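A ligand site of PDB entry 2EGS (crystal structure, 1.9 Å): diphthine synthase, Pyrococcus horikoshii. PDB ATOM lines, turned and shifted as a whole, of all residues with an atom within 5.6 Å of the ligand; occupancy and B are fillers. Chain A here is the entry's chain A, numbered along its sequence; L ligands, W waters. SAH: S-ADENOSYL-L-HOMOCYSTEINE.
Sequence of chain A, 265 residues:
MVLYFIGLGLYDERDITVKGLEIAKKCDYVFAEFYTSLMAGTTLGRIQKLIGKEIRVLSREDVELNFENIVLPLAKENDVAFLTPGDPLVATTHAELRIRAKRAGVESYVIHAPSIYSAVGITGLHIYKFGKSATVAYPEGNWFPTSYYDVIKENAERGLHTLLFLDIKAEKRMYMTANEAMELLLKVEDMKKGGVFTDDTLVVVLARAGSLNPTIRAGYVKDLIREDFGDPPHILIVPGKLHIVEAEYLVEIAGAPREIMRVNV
N of Tyr 117 sits close to OG of Ser 115 (3.2 Å). The side-chain carboxylate of Asp 87 is in hydrogen-bond range of the backbone NH of Leu 89 (2.9 Å). O of Leu 206 sits at hydrogen-bond distance from N of Ile 235 (3.0 Å). The backbone NH (N) of Arg 208 sits at hydrogen-bond distance from the backbone carbonyl oxygen (O) of Pro 233. The side-chain hydroxyl (OG1) of Thr 92 lies within hydrogen-bond range of the backbone carbonyl oxygen (O) of Pro 88.
The backbone carbonyl oxygen (O) of Thr 36 sits close to a sulfur (SD) of the ligand (3.6 Å). Ser 37 touches the ligand (OG to C8, 3.2 Å). Gly 86 touches the ligand. Ala 91 touches the ligand. Thr 92 touches the ligand (CG2 to N, 3.8 Å). CD1 of Phe 165 touches O4' of the ligand, at 3.6 Å. Leu 206 touches the ligand (O to C2, 3.7 Å). Pro 233 touches the ligand. Ile 235 touches the ligand. Hydrophobic or aromatic side chains within 4 Å of the ligand: Leu 10, Val 90, Ala 91, Ile 116, Phe 165, Leu 166, Ala 209, Pro 233 and Ile 235. Of the 30 residues printed, 18 come within 4 Å of the ligand. Along chain A the residues within 4 Å of the ligand span positions 10 to 235.
Water W4 lies within hydrogen-bond range of the side-chain hydroxyl (OG1) of Thr 36, a nitrogen (N) of the ligand and the backbone carbonyl oxygen (O) of Pro 85. Water W3 bridges an oxygen (O3') of the ligand (2.8 Å) and the backbone carbonyl oxygen of Asp 167 (2.9 Å).
A nitrogen (N) of the ligand lies within hydrogen-bond range of the backbone carbonyl oxygen (O) of Val 90. The backbone carbonyl oxygen (O) of His 234 lies within hydrogen-bond range of an oxygen (O2') of the ligand (2.6 Å). The backbone NH of Leu 166 sits at hydrogen-bond distance from an oxygen (O2') of the ligand, 2.9 Å away. An oxygen (O3') of the ligand lies within hydrogen-bond range of the backbone carbonyl oxygen (O) of Leu 166, at 2.7 Å. N of Ala 209 sits at hydrogen-bond distance from N1 of the ligand, 3.0 Å away. O of Ala 209 lies within hydrogen-bond range of N6 of the ligand, 2.7 Å away. OG of Ser 115 lies within hydrogen-bond range of O of the ligand, at 2.7 Å. The backbone NH (N) of Asp 87 lies within hydrogen-bond range of an oxygen (O) of the ligand. The backbone carbonyl oxygen of Asp 87 is in hydrogen-bond range of a nitrogen (N) of the ligand (2.8 Å). The backbone NH (N) of Ile 116 is in hydrogen-bond range of an oxygen (OXT) of the ligand (3.0 Å). The backbone carbonyl oxygen of Leu 10 sits at hydrogen-bond distance from a nitrogen (N6) of the ligand (3.2 Å). The backbone NH (N) of Arg 208 lies within hydrogen-bond range of a nitrogen (N1) of the ligand.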
ATOM      1  N   LEU A  10     -22.056 -30.445  -6.334  1.00  0.00           N
ATOM      2  CA  LEU A  10     -22.876 -29.255  -6.149  1.00  0.00           C
ATOM      3  C   LEU A  10     -23.808 -28.690  -7.213  1.00  0.00           C
ATOM      4  O   LEU A  10     -24.923 -28.286  -6.884  1.00  0.00           O
ATOM      5  CB  LEU A  10     -21.960 -28.108  -5.744  1.00  0.00           C
ATOM      6  CG  LEU A  10     -21.000 -28.355  -4.572  1.00  0.00           C
ATOM      7  CD1 LEU A  10     -19.952 -27.261  -4.542  1.00  0.00           C
ATOM      8  CD2 LEU A  10     -21.785 -28.417  -3.276  1.00  0.00           C
ATOM      9  N   TYR A  11     -23.356 -28.658  -8.463  1.00  0.00           N
ATOM     10  CA  TYR A  11     -24.143 -27.996  -9.492  1.00  0.00           C
ATOM     11  C   TYR A  11     -24.384 -28.756 -10.808  1.00  0.00           C
ATOM     12  O   TYR A  11     -25.526 -28.895 -11.233  1.00  0.00           O
ATOM     13  CB  TYR A  11     -23.459 -26.652  -9.774  1.00  0.00           C
ATOM     14  CG  TYR A  11     -24.160 -25.727 -10.732  1.00  0.00           C
ATOM     15  CD1 TYR A  11     -25.334 -25.065 -10.373  1.00  0.00           C
ATOM     16  CD2 TYR A  11     -23.630 -25.483 -11.998  1.00  0.00           C
ATOM     17  CE1 TYR A  11     -25.959 -24.178 -11.248  1.00  0.00           C
ATOM     18  CE2 TYR A  11     -24.251 -24.610 -12.891  1.00  0.00           C
ATOM     19  CZ  TYR A  11     -25.413 -23.956 -12.505  1.00  0.00           C
ATOM     20  OH  TYR A  11     -26.019 -23.093 -13.382  1.00  0.00           O
ATOM     21  N   THR A  36     -32.719 -35.055  -2.141  1.00  0.00           N
ATOM     22  CA  THR A  36     -32.002 -34.497  -0.998  1.00  0.00           C
ATOM     23  C   THR A  36     -31.432 -33.122  -1.309  1.00  0.00           C
ATOM     24  O   THR A  36     -31.105 -32.352  -0.403  1.00  0.00           O
ATOM     25  CB  THR A  36     -30.846 -35.413  -0.523  1.00  0.00           C
ATOM     26  OG1 THR A  36     -29.985 -35.722  -1.632  1.00  0.00           O
ATOM     27  CG2 THR A  36     -31.398 -36.700   0.062  1.00  0.00           C
ATOM     28  N   SER A  37     -31.300 -32.795  -2.590  1.00  0.00           N
ATOM     29  CA  SER A  37     -30.785 -31.496  -2.986  1.00  0.00           C
ATOM     30  C   SER A  37     -31.096 -31.227  -4.450  1.00  0.00           C
ATOM     31  O   SER A  37     -31.701 -32.057  -5.118  1.00  0.00           O
ATOM     32  CB  SER A  37     -29.263 -31.448  -2.762  1.00  0.00           C
ATOM     33  OG  SER A  37     -28.763 -30.144  -3.006  1.00  0.00           O
ATOM     34  N   LEU A  38     -30.675 -30.069  -4.922  1.00  0.00           N
ATOM     35  CA  LEU A  38     -30.914 -29.665  -6.305  1.00  0.00           C
ATOM     36  C   LEU A  38     -29.645 -29.319  -7.077  1.00  0.00           C
ATOM     37  O   LEU A  38     -28.862 -28.460  -6.669  1.00  0.00           O
ATOM     38  CB  LEU A  38     -31.861 -28.461  -6.349  1.00  0.00           C
ATOM     39  CG  LEU A  38     -32.134 -27.882  -7.742  1.00  0.00           C
ATOM     40  CD1 LEU A  38     -32.917 -28.893  -8.567  1.00  0.00           C
ATOM     41  CD2 LEU A  38     -32.913 -26.574  -7.619  1.00  0.00           C
ATOM     42  N   PRO A  85     -26.880 -36.025  -5.071  1.00  0.00           N
ATOM     43  CA  PRO A  85     -26.313 -34.701  -5.319  1.00  0.00           C
ATOM     44  C   PRO A  85     -25.289 -34.455  -4.209  1.00  0.00           C
ATOM     45  O   PRO A  85     -25.355 -35.122  -3.173  1.00  0.00           O
ATOM     46  CB  PRO A  85     -27.519 -33.772  -5.188  1.00  0.00           C
ATOM     47  CG  PRO A  85     -28.693 -34.649  -5.527  1.00  0.00           C
ATOM     48  CD  PRO A  85     -28.338 -35.956  -4.853  1.00  0.00           C
ATOM     49  N   GLY A  86     -24.373 -33.519  -4.411  1.00  0.00           N
ATOM     50  CA  GLY A  86     -23.365 -33.215  -3.400  1.00  0.00           C
ATOM     51  C   GLY A  86     -22.643 -34.430  -2.869  1.00  0.00           C
ATOM     52  O   GLY A  86     -22.260 -35.300  -3.654  1.00  0.00           O
ATOM     53  N   ASP A  87     -22.433 -34.483  -1.560  1.00  0.00           N
ATOM     54  CA  ASP A  87     -21.784 -35.619  -0.906  1.00  0.00           C
ATOM     55  C   ASP A  87     -22.925 -36.484  -0.360  1.00  0.00           C
ATOM     56  O   ASP A  87     -23.819 -35.986   0.334  1.00  0.00           O
ATOM     57  CB  ASP A  87     -20.870 -35.141   0.225  1.00  0.00           C
ATOM     58  CG  ASP A  87     -20.129 -36.279   0.885  1.00  0.00           C
ATOM     59  OD1 ASP A  87     -20.780 -37.102   1.556  1.00  0.00           O
ATOM     60  OD2 ASP A  87     -18.879 -36.340   0.732  1.00  0.00           O
ATOM     61  N   PRO A  88     -22.912 -37.783  -0.655  1.00  0.00           N
ATOM     62  CA  PRO A  88     -23.955 -38.707  -0.207  1.00  0.00           C
ATOM     63  C   PRO A  88     -24.269 -38.815   1.287  1.00  0.00           C
ATOM     64  O   PRO A  88     -25.373 -39.202   1.650  1.00  0.00           O
ATOM     65  CB  PRO A  88     -23.516 -40.047  -0.804  1.00  0.00           C
ATOM     66  CG  PRO A  88     -22.030 -39.915  -0.881  1.00  0.00           C
ATOM     67  CD  PRO A  88     -21.820 -38.512  -1.344  1.00  0.00           C
ATOM     68  N   LEU A  89     -23.311 -38.456   2.136  1.00  0.00           N
ATOM     69  CA  LEU A  89     -23.526 -38.574   3.576  1.00  0.00           C
ATOM     70  C   LEU A  89     -23.601 -37.259   4.348  1.00  0.00           C
ATOM     71  O   LEU A  89     -23.499 -37.257   5.583  1.00  0.00           O
ATOM     72  CB  LEU A  89     -22.417 -39.433   4.186  1.00  0.00           C
ATOM     73  CG  LEU A  89     -22.174 -40.772   3.479  1.00  0.00           C
ATOM     74  CD1 LEU A  89     -21.068 -41.523   4.195  1.00  0.00           C
ATOM     75  CD2 LEU A  89     -23.448 -41.581   3.447  1.00  0.00           C
ATOM     76  N   VAL A  90     -23.764 -36.156   3.641  1.00  0.00           N
ATOM     77  CA  VAL A  90     -23.857 -34.856   4.294  1.00  0.00           C
ATOM     78  C   VAL A  90     -25.294 -34.347   4.267  1.00  0.00           C
ATOM     79  O   VAL A  90     -25.870 -34.158   3.196  1.00  0.00           O
ATOM     80  CB  VAL A  90     -22.949 -33.816   3.605  1.00  0.00           C
ATOM     81  CG1 VAL A  90     -23.209 -32.422   4.181  1.00  0.00           C
ATOM     82  CG2 VAL A  90     -21.487 -34.192   3.794  1.00  0.00           C
ATOM     83  N   ALA A  91     -25.869 -34.128   5.444  1.00  0.00           N
ATOM     84  CA  ALA A  91     -27.230 -33.621   5.545  1.00  0.00           C
ATOM     85  C   ALA A  91     -28.252 -34.536   4.876  1.00  0.00           C
ATOM     86  O   ALA A  91     -29.217 -34.064   4.264  1.00  0.00           O
ATOM     87  CB  ALA A  91     -27.304 -32.219   4.947  1.00  0.00           C
ATOM     88  N   THR A  92     -28.014 -35.839   4.975  1.00  0.00           N
ATOM     89  CA  THR A  92     -28.933 -36.861   4.515  1.00  0.00           C
ATOM     90  C   THR A  92     -29.005 -37.940   5.583  1.00  0.00           C
ATOM     91  O   THR A  92     -28.329 -37.884   6.606  1.00  0.00           O
ATOM     92  CB  THR A  92     -28.406 -37.470   3.206  1.00  0.00           C
ATOM     93  OG1 THR A  92     -27.259 -38.282   3.469  1.00  0.00           O
ATOM     94  CG2 THR A  92     -28.026 -36.372   2.203  1.00  0.00           C
ATOM     95  N   PRO A 114     -17.880 -32.691  -3.958  1.00  0.00           N
ATOM     96  CA  PRO A 114     -17.996 -31.370  -3.327  1.00  0.00           C
ATOM     97  C   PRO A 114     -19.341 -31.251  -2.578  1.00  0.00           C
ATOM     98  O   PRO A 114     -20.376 -31.662  -3.090  1.00  0.00           O
ATOM     99  CB  PRO A 114     -17.920 -30.410  -4.509  1.00  0.00           C
ATOM    100  CG  PRO A 114     -17.127 -31.167  -5.533  1.00  0.00           C
ATOM    101  CD  PRO A 114     -17.634 -32.577  -5.399  1.00  0.00           C
ATOM    102  N   SER A 115     -19.297 -30.703  -1.365  1.00  0.00           N
ATOM    103  CA  SER A 115     -20.492 -30.543  -0.548  1.00  0.00           C
ATOM    104  C   SER A 115     -20.740 -29.081  -0.192  1.00  0.00           C
ATOM    105  O   SER A 115     -19.801 -28.306  -0.009  1.00  0.00           O
ATOM    106  CB  SER A 115     -20.346 -31.355   0.746  1.00  0.00           C
ATOM    107  OG  SER A 115     -21.416 -31.090   1.633  1.00  0.00           O
ATOM    108  N   ILE A 116     -22.009 -28.698  -0.084  1.00  0.00           N
ATOM    109  CA  ILE A 116     -22.327 -27.319   0.266  1.00  0.00           C
ATOM    110  C   ILE A 116     -21.771 -26.989   1.659  1.00  0.00           C
ATOM    111  O   ILE A 116     -21.429 -25.841   1.948  1.00  0.00           O
ATOM    112  CB  ILE A 116     -23.841 -27.069   0.275  1.00  0.00           C
ATOM    113  CG1 ILE A 116     -24.116 -25.578   0.522  1.00  0.00           C
ATOM    114  CG2 ILE A 116     -24.497 -27.901   1.370  1.00  0.00           C
ATOM    115  CD1 ILE A 116     -23.568 -24.680  -0.574  1.00  0.00           C
ATOM    116  N   TYR A 117     -21.686 -28.009   2.507  1.00  0.00           N
ATOM    117  CA  TYR A 117     -21.185 -27.841   3.860  1.00  0.00           C
ATOM    118  C   TYR A 117     -19.762 -27.258   3.882  1.00  0.00           C
ATOM    119  O   TYR A 117     -19.421 -26.481   4.780  1.00  0.00           O
ATOM    120  CB  TYR A 117     -21.259 -29.184   4.584  1.00  0.00           C
ATOM    121  CG  TYR A 117     -20.836 -29.173   6.039  1.00  0.00           C
ATOM    122  CD1 TYR A 117     -21.553 -28.476   7.002  1.00  0.00           C
ATOM    123  CD2 TYR A 117     -19.717 -29.909   6.450  1.00  0.00           C
ATOM    124  CE1 TYR A 117     -21.173 -28.507   8.347  1.00  0.00           C
ATOM    125  CE2 TYR A 117     -19.336 -29.951   7.786  1.00  0.00           C
ATOM    126  CZ  TYR A 117     -20.069 -29.255   8.733  1.00  0.00           C
ATOM    127  OH  TYR A 117     -19.671 -29.312  10.045  1.00  0.00           O
ATOM    128  N   LEU A 164     -27.268 -22.381   7.421  1.00  0.00           N
ATOM    129  CA  LEU A 164     -28.669 -22.755   7.388  1.00  0.00           C
ATOM    130  C   LEU A 164     -29.040 -23.424   6.081  1.00  0.00           C
ATOM    131  O   LEU A 164     -29.154 -22.763   5.047  1.00  0.00           O
ATOM    132  CB  LEU A 164     -29.563 -21.533   7.588  1.00  0.00           C
ATOM    133  CG  LEU A 164     -29.453 -20.795   8.912  1.00  0.00           C
ATOM    134  CD1 LEU A 164     -30.206 -19.471   8.818  1.00  0.00           C
ATOM    135  CD2 LEU A 164     -30.004 -21.648  10.031  1.00  0.00           C
ATOM    136  N   PHE A 165     -29.205 -24.742   6.118  1.00  0.00           N
ATOM    137  CA  PHE A 165     -29.617 -25.509   4.944  1.00  0.00           C
ATOM    138  C   PHE A 165     -31.070 -25.073   4.746  1.00  0.00           C
ATOM    139  O   PHE A 165     -31.786 -24.895   5.720  1.00  0.00           O
ATOM    140  CB  PHE A 165     -29.586 -26.998   5.250  1.00  0.00           C
ATOM    141  CG  PHE A 165     -28.194 -27.558   5.443  1.00  0.00           C
ATOM    142  CD1 PHE A 165     -27.404 -27.875   4.357  1.00  0.00           C
ATOM    143  CD2 PHE A 165     -27.695 -27.757   6.726  1.00  0.00           C
ATOM    144  CE1 PHE A 165     -26.119 -28.393   4.532  1.00  0.00           C
ATOM    145  CE2 PHE A 165     -26.407 -28.282   6.924  1.00  0.00           C
ATOM    146  CZ  PHE A 165     -25.624 -28.599   5.825  1.00  0.00           C
ATOM    147  N   LEU A 166     -31.496 -24.901   3.489  1.00  0.00           N
ATOM    148  CA  LEU A 166     -32.872 -24.474   3.241  1.00  0.00           C
ATOM    149  C   LEU A 166     -33.723 -25.646   2.722  1.00  0.00           C
ATOM    150  O   LEU A 166     -33.256 -26.517   2.004  1.00  0.00           O
ATOM    151  CB  LEU A 166     -32.845 -23.354   2.195  1.00  0.00           C
ATOM    152  CG  LEU A 166     -32.031 -22.147   2.643  1.00  0.00           C
ATOM    153  CD1 LEU A 166     -32.232 -20.938   1.715  1.00  0.00           C
ATOM    154  CD2 LEU A 166     -32.389 -21.659   4.046  1.00  0.00           C
ATOM    155  N   ASP A 167     -34.997 -25.656   3.135  1.00  0.00           N
ATOM    156  CA  ASP A 167     -35.810 -26.833   2.830  1.00  0.00           C
ATOM    157  C   ASP A 167     -36.030 -27.002   1.316  1.00  0.00           C
ATOM    158  O   ASP A 167     -35.848 -26.092   0.523  1.00  0.00           O
ATOM    159  CB  ASP A 167     -37.164 -26.680   3.517  1.00  0.00           C
ATOM    160  CG  ASP A 167     -37.816 -28.039   3.726  1.00  0.00           C
ATOM    161  OD1 ASP A 167     -37.313 -29.016   3.165  1.00  0.00           O
ATOM    162  OD2 ASP A 167     -38.819 -28.116   4.432  1.00  0.00           O
ATOM    163  N   ILE A 168     -36.358 -28.271   0.979  1.00  0.00           N
ATOM    164  CA  ILE A 168     -36.635 -28.617  -0.403  1.00  0.00           C
ATOM    165  C   ILE A 168     -37.770 -29.644  -0.471  1.00  0.00           C
ATOM    166  O   ILE A 168     -37.923 -30.498   0.383  1.00  0.00           O
ATOM    167  CB  ILE A 168     -35.372 -29.233  -1.000  1.00  0.00           C
ATOM    168  CG1 ILE A 168     -35.668 -29.850  -2.369  1.00  0.00           C
ATOM    169  CG2 ILE A 168     -34.856 -30.353  -0.081  1.00  0.00           C
ATOM    170  CD1 ILE A 168     -34.400 -30.368  -3.056  1.00  0.00           C
ATOM    171  N   LEU A 206     -25.463 -17.619  -0.361  1.00  0.00           N
ATOM    172  CA  LEU A 206     -24.678 -18.301  -1.370  1.00  0.00           C
ATOM    173  C   LEU A 206     -25.686 -19.060  -2.212  1.00  0.00           C
ATOM    174  O   LEU A 206     -26.414 -19.907  -1.707  1.00  0.00           O
ATOM    175  CB  LEU A 206     -23.689 -19.290  -0.718  1.00  0.00           C
ATOM    176  CG  LEU A 206     -22.855 -20.155  -1.669  1.00  0.00           C
ATOM    177  CD1 LEU A 206     -22.065 -19.281  -2.637  1.00  0.00           C
ATOM    178  CD2 LEU A 206     -21.909 -21.021  -0.841  1.00  0.00           C
ATOM    179  N   ALA A 207     -25.742 -18.729  -3.496  1.00  0.00           N
ATOM    180  CA  ALA A 207     -26.694 -19.380  -4.383  1.00  0.00           C
ATOM    181  C   ALA A 207     -25.984 -20.082  -5.528  1.00  0.00           C
ATOM    182  O   ALA A 207     -25.088 -19.520  -6.153  1.00  0.00           O
ATOM    183  CB  ALA A 207     -27.686 -18.357  -4.947  1.00  0.00           C
ATOM    184  N   ARG A 208     -26.400 -21.326  -5.779  1.00  0.00           N
ATOM    185  CA  ARG A 208     -25.828 -22.130  -6.849  1.00  0.00           C
ATOM    186  C   ARG A 208     -24.324 -22.310  -6.736  1.00  0.00           C
ATOM    187  O   ARG A 208     -23.577 -22.061  -7.685  1.00  0.00           O
ATOM    188  CB  ARG A 208     -26.179 -21.505  -8.210  1.00  0.00           C
ATOM    189  CG  ARG A 208     -27.688 -21.407  -8.468  1.00  0.00           C
ATOM    190  CD  ARG A 208     -27.969 -20.694  -9.793  1.00  0.00           C
ATOM    191  NE  ARG A 208     -27.268 -19.421  -9.845  1.00  0.00           N
ATOM    192  CZ  ARG A 208     -27.581 -18.362  -9.095  1.00  0.00           C
ATOM    193  NH1 ARG A 208     -28.604 -18.425  -8.250  1.00  0.00           N
ATOM    194  NH2 ARG A 208     -26.847 -17.260  -9.170  1.00  0.00           N
ATOM    195  N   ALA A 209     -23.866 -22.721  -5.553  1.00  0.00           N
ATOM    196  CA  ALA A 209     -22.451 -22.977  -5.346  1.00  0.00           C
ATOM    197  C   ALA A 209     -22.113 -24.094  -6.331  1.00  0.00           C
ATOM    198  O   ALA A 209     -22.959 -24.945  -6.601  1.00  0.00           O
ATOM    199  CB  ALA A 209     -22.209 -23.435  -3.920  1.00  0.00           C
ATOM    200  N   GLY A 210     -20.901 -24.101  -6.854  1.00  0.00           N
ATOM    201  CA  GLY A 210     -20.529 -25.118  -7.816  1.00  0.00           C
ATOM    202  C   GLY A 210     -20.494 -24.552  -9.223  1.00  0.00           C
ATOM    203  O   GLY A 210     -19.685 -24.956 -10.055  1.00  0.00           O
ATOM    204  N   PRO A 233     -30.452 -23.873  -6.004  1.00  0.00           N
ATOM    205  CA  PRO A 233     -30.641 -23.880  -4.545  1.00  0.00           C
ATOM    206  C   PRO A 233     -29.940 -22.707  -3.880  1.00  0.00           C
ATOM    207  O   PRO A 233     -29.002 -22.130  -4.432  1.00  0.00           O
ATOM    208  CB  PRO A 233     -30.041 -25.217  -4.133  1.00  0.00           C
ATOM    209  CG  PRO A 233     -28.889 -25.339  -5.075  1.00  0.00           C
ATOM    210  CD  PRO A 233     -29.466 -24.892  -6.406  1.00  0.00           C
ATOM    211  N   HIS A 234     -30.396 -22.368  -2.679  1.00  0.00           N
ATOM    212  CA  HIS A 234     -29.828 -21.274  -1.912  1.00  0.00           C
ATOM    213  C   HIS A 234     -29.447 -21.780  -0.543  1.00  0.00           C
ATOM    214  O   HIS A 234     -30.014 -22.753  -0.052  1.00  0.00           O
ATOM    215  CB  HIS A 234     -30.854 -20.143  -1.691  1.00  0.00           C
ATOM    216  CG  HIS A 234     -31.201 -19.345  -2.913  1.00  0.00           C
ATOM    217  ND1 HIS A 234     -31.998 -18.228  -2.856  1.00  0.00           N
ATOM    218  CD2 HIS A 234     -30.857 -19.509  -4.211  1.00  0.00           C
ATOM    219  CE1 HIS A 234     -32.131 -17.724  -4.078  1.00  0.00           C
ATOM    220  NE2 HIS A 234     -31.459 -18.488  -4.914  1.00  0.00           N
ATOM    221  N   ILE A 235     -28.494 -21.107   0.076  1.00  0.00           N
ATOM    222  CA  ILE A 235     -28.092 -21.435   1.429  1.00  0.00           C
ATOM    223  C   ILE A 235     -27.982 -20.090   2.154  1.00  0.00           C
ATOM    224  O   ILE A 235     -27.531 -19.116   1.566  1.00  0.00           O
ATOM    225  CB  ILE A 235     -26.744 -22.195   1.466  1.00  0.00           C
ATOM    226  CG1 ILE A 235     -26.618 -22.962   2.767  1.00  0.00           C
ATOM    227  CG2 ILE A 235     -25.574 -21.233   1.334  1.00  0.00           C
ATOM    228  CD1 ILE A 235     -27.560 -24.137   2.847  1.00  0.00           C
HETATM  229  N   SAH L   1     -25.594 -33.881   0.654  1.00  0.00           N
HETATM  230  CA  SAH L   1     -25.794 -32.467   0.090  1.00  0.00           C
HETATM  231  CB  SAH L   1     -26.689 -31.558   0.877  1.00  0.00           C
HETATM  232  CG  SAH L   1     -28.123 -31.986   1.141  1.00  0.00           C
HETATM  233  SD  SAH L   1     -28.975 -30.560   1.940  1.00  0.00           S
HETATM  234  C   SAH L   1     -24.354 -31.830  -0.062  1.00  0.00           C
HETATM  235  O   SAH L   1     -23.358 -32.497   0.289  1.00  0.00           O
HETATM  236  OXT SAH L   1     -24.304 -30.632  -0.544  1.00  0.00           O
HETATM  237  C5' SAH L   1     -29.553 -29.717   0.525  1.00  0.00           C
HETATM  238  C4' SAH L   1     -29.632 -28.157   0.806  1.00  0.00           C
HETATM  239  O4' SAH L   1     -28.266 -27.648   0.889  1.00  0.00           O
HETATM  240  C3' SAH L   1     -30.305 -27.361  -0.247  1.00  0.00           C
HETATM  241  O3' SAH L   1     -31.698 -27.308  -0.008  1.00  0.00           O
HETATM  242  C2' SAH L   1     -29.574 -26.007  -0.136  1.00  0.00           C
HETATM  243  O2' SAH L   1     -30.092 -25.210   0.930  1.00  0.00           O
HETATM  244  C1' SAH L   1     -28.111 -26.400   0.079  1.00  0.00           C
HETATM  245  N9  SAH L   1     -27.405 -26.651  -1.055  1.00  0.00           N
HETATM  246  C8  SAH L   1     -26.997 -27.794  -1.729  1.00  0.00           C
HETATM  247  N7  SAH L   1     -26.316 -27.587  -2.817  1.00  0.00           N
HETATM  248  C5  SAH L   1     -26.240 -26.163  -2.911  1.00  0.00           C
HETATM  249  C6  SAH L   1     -25.616 -25.309  -3.892  1.00  0.00           C
HETATM  250  N6  SAH L   1     -24.946 -25.751  -4.968  1.00  0.00           N
HETATM  251  N1  SAH L   1     -25.755 -23.961  -3.653  1.00  0.00           N
HETATM  252  C2  SAH L   1     -26.430 -23.457  -2.578  1.00  0.00           C
HETATM  253  N3  SAH L   1     -27.038 -24.245  -1.626  1.00  0.00           N
HETATM  254  C4  SAH L   1     -26.901 -25.583  -1.857  1.00  0.00           C
HETATM  255  O   HOH W   1     -24.810 -29.926  -3.320  1.00  0.00           O
HETATM  256  O   HOH W   2     -26.857 -30.249  -5.022  1.00  0.00           O
HETATM  257  O   HOH W   3     -33.690 -25.929  -1.448  1.00  0.00           O
HETATM  258  O   HOH W   4     -27.447 -34.730  -1.254  1.00  0.00           O
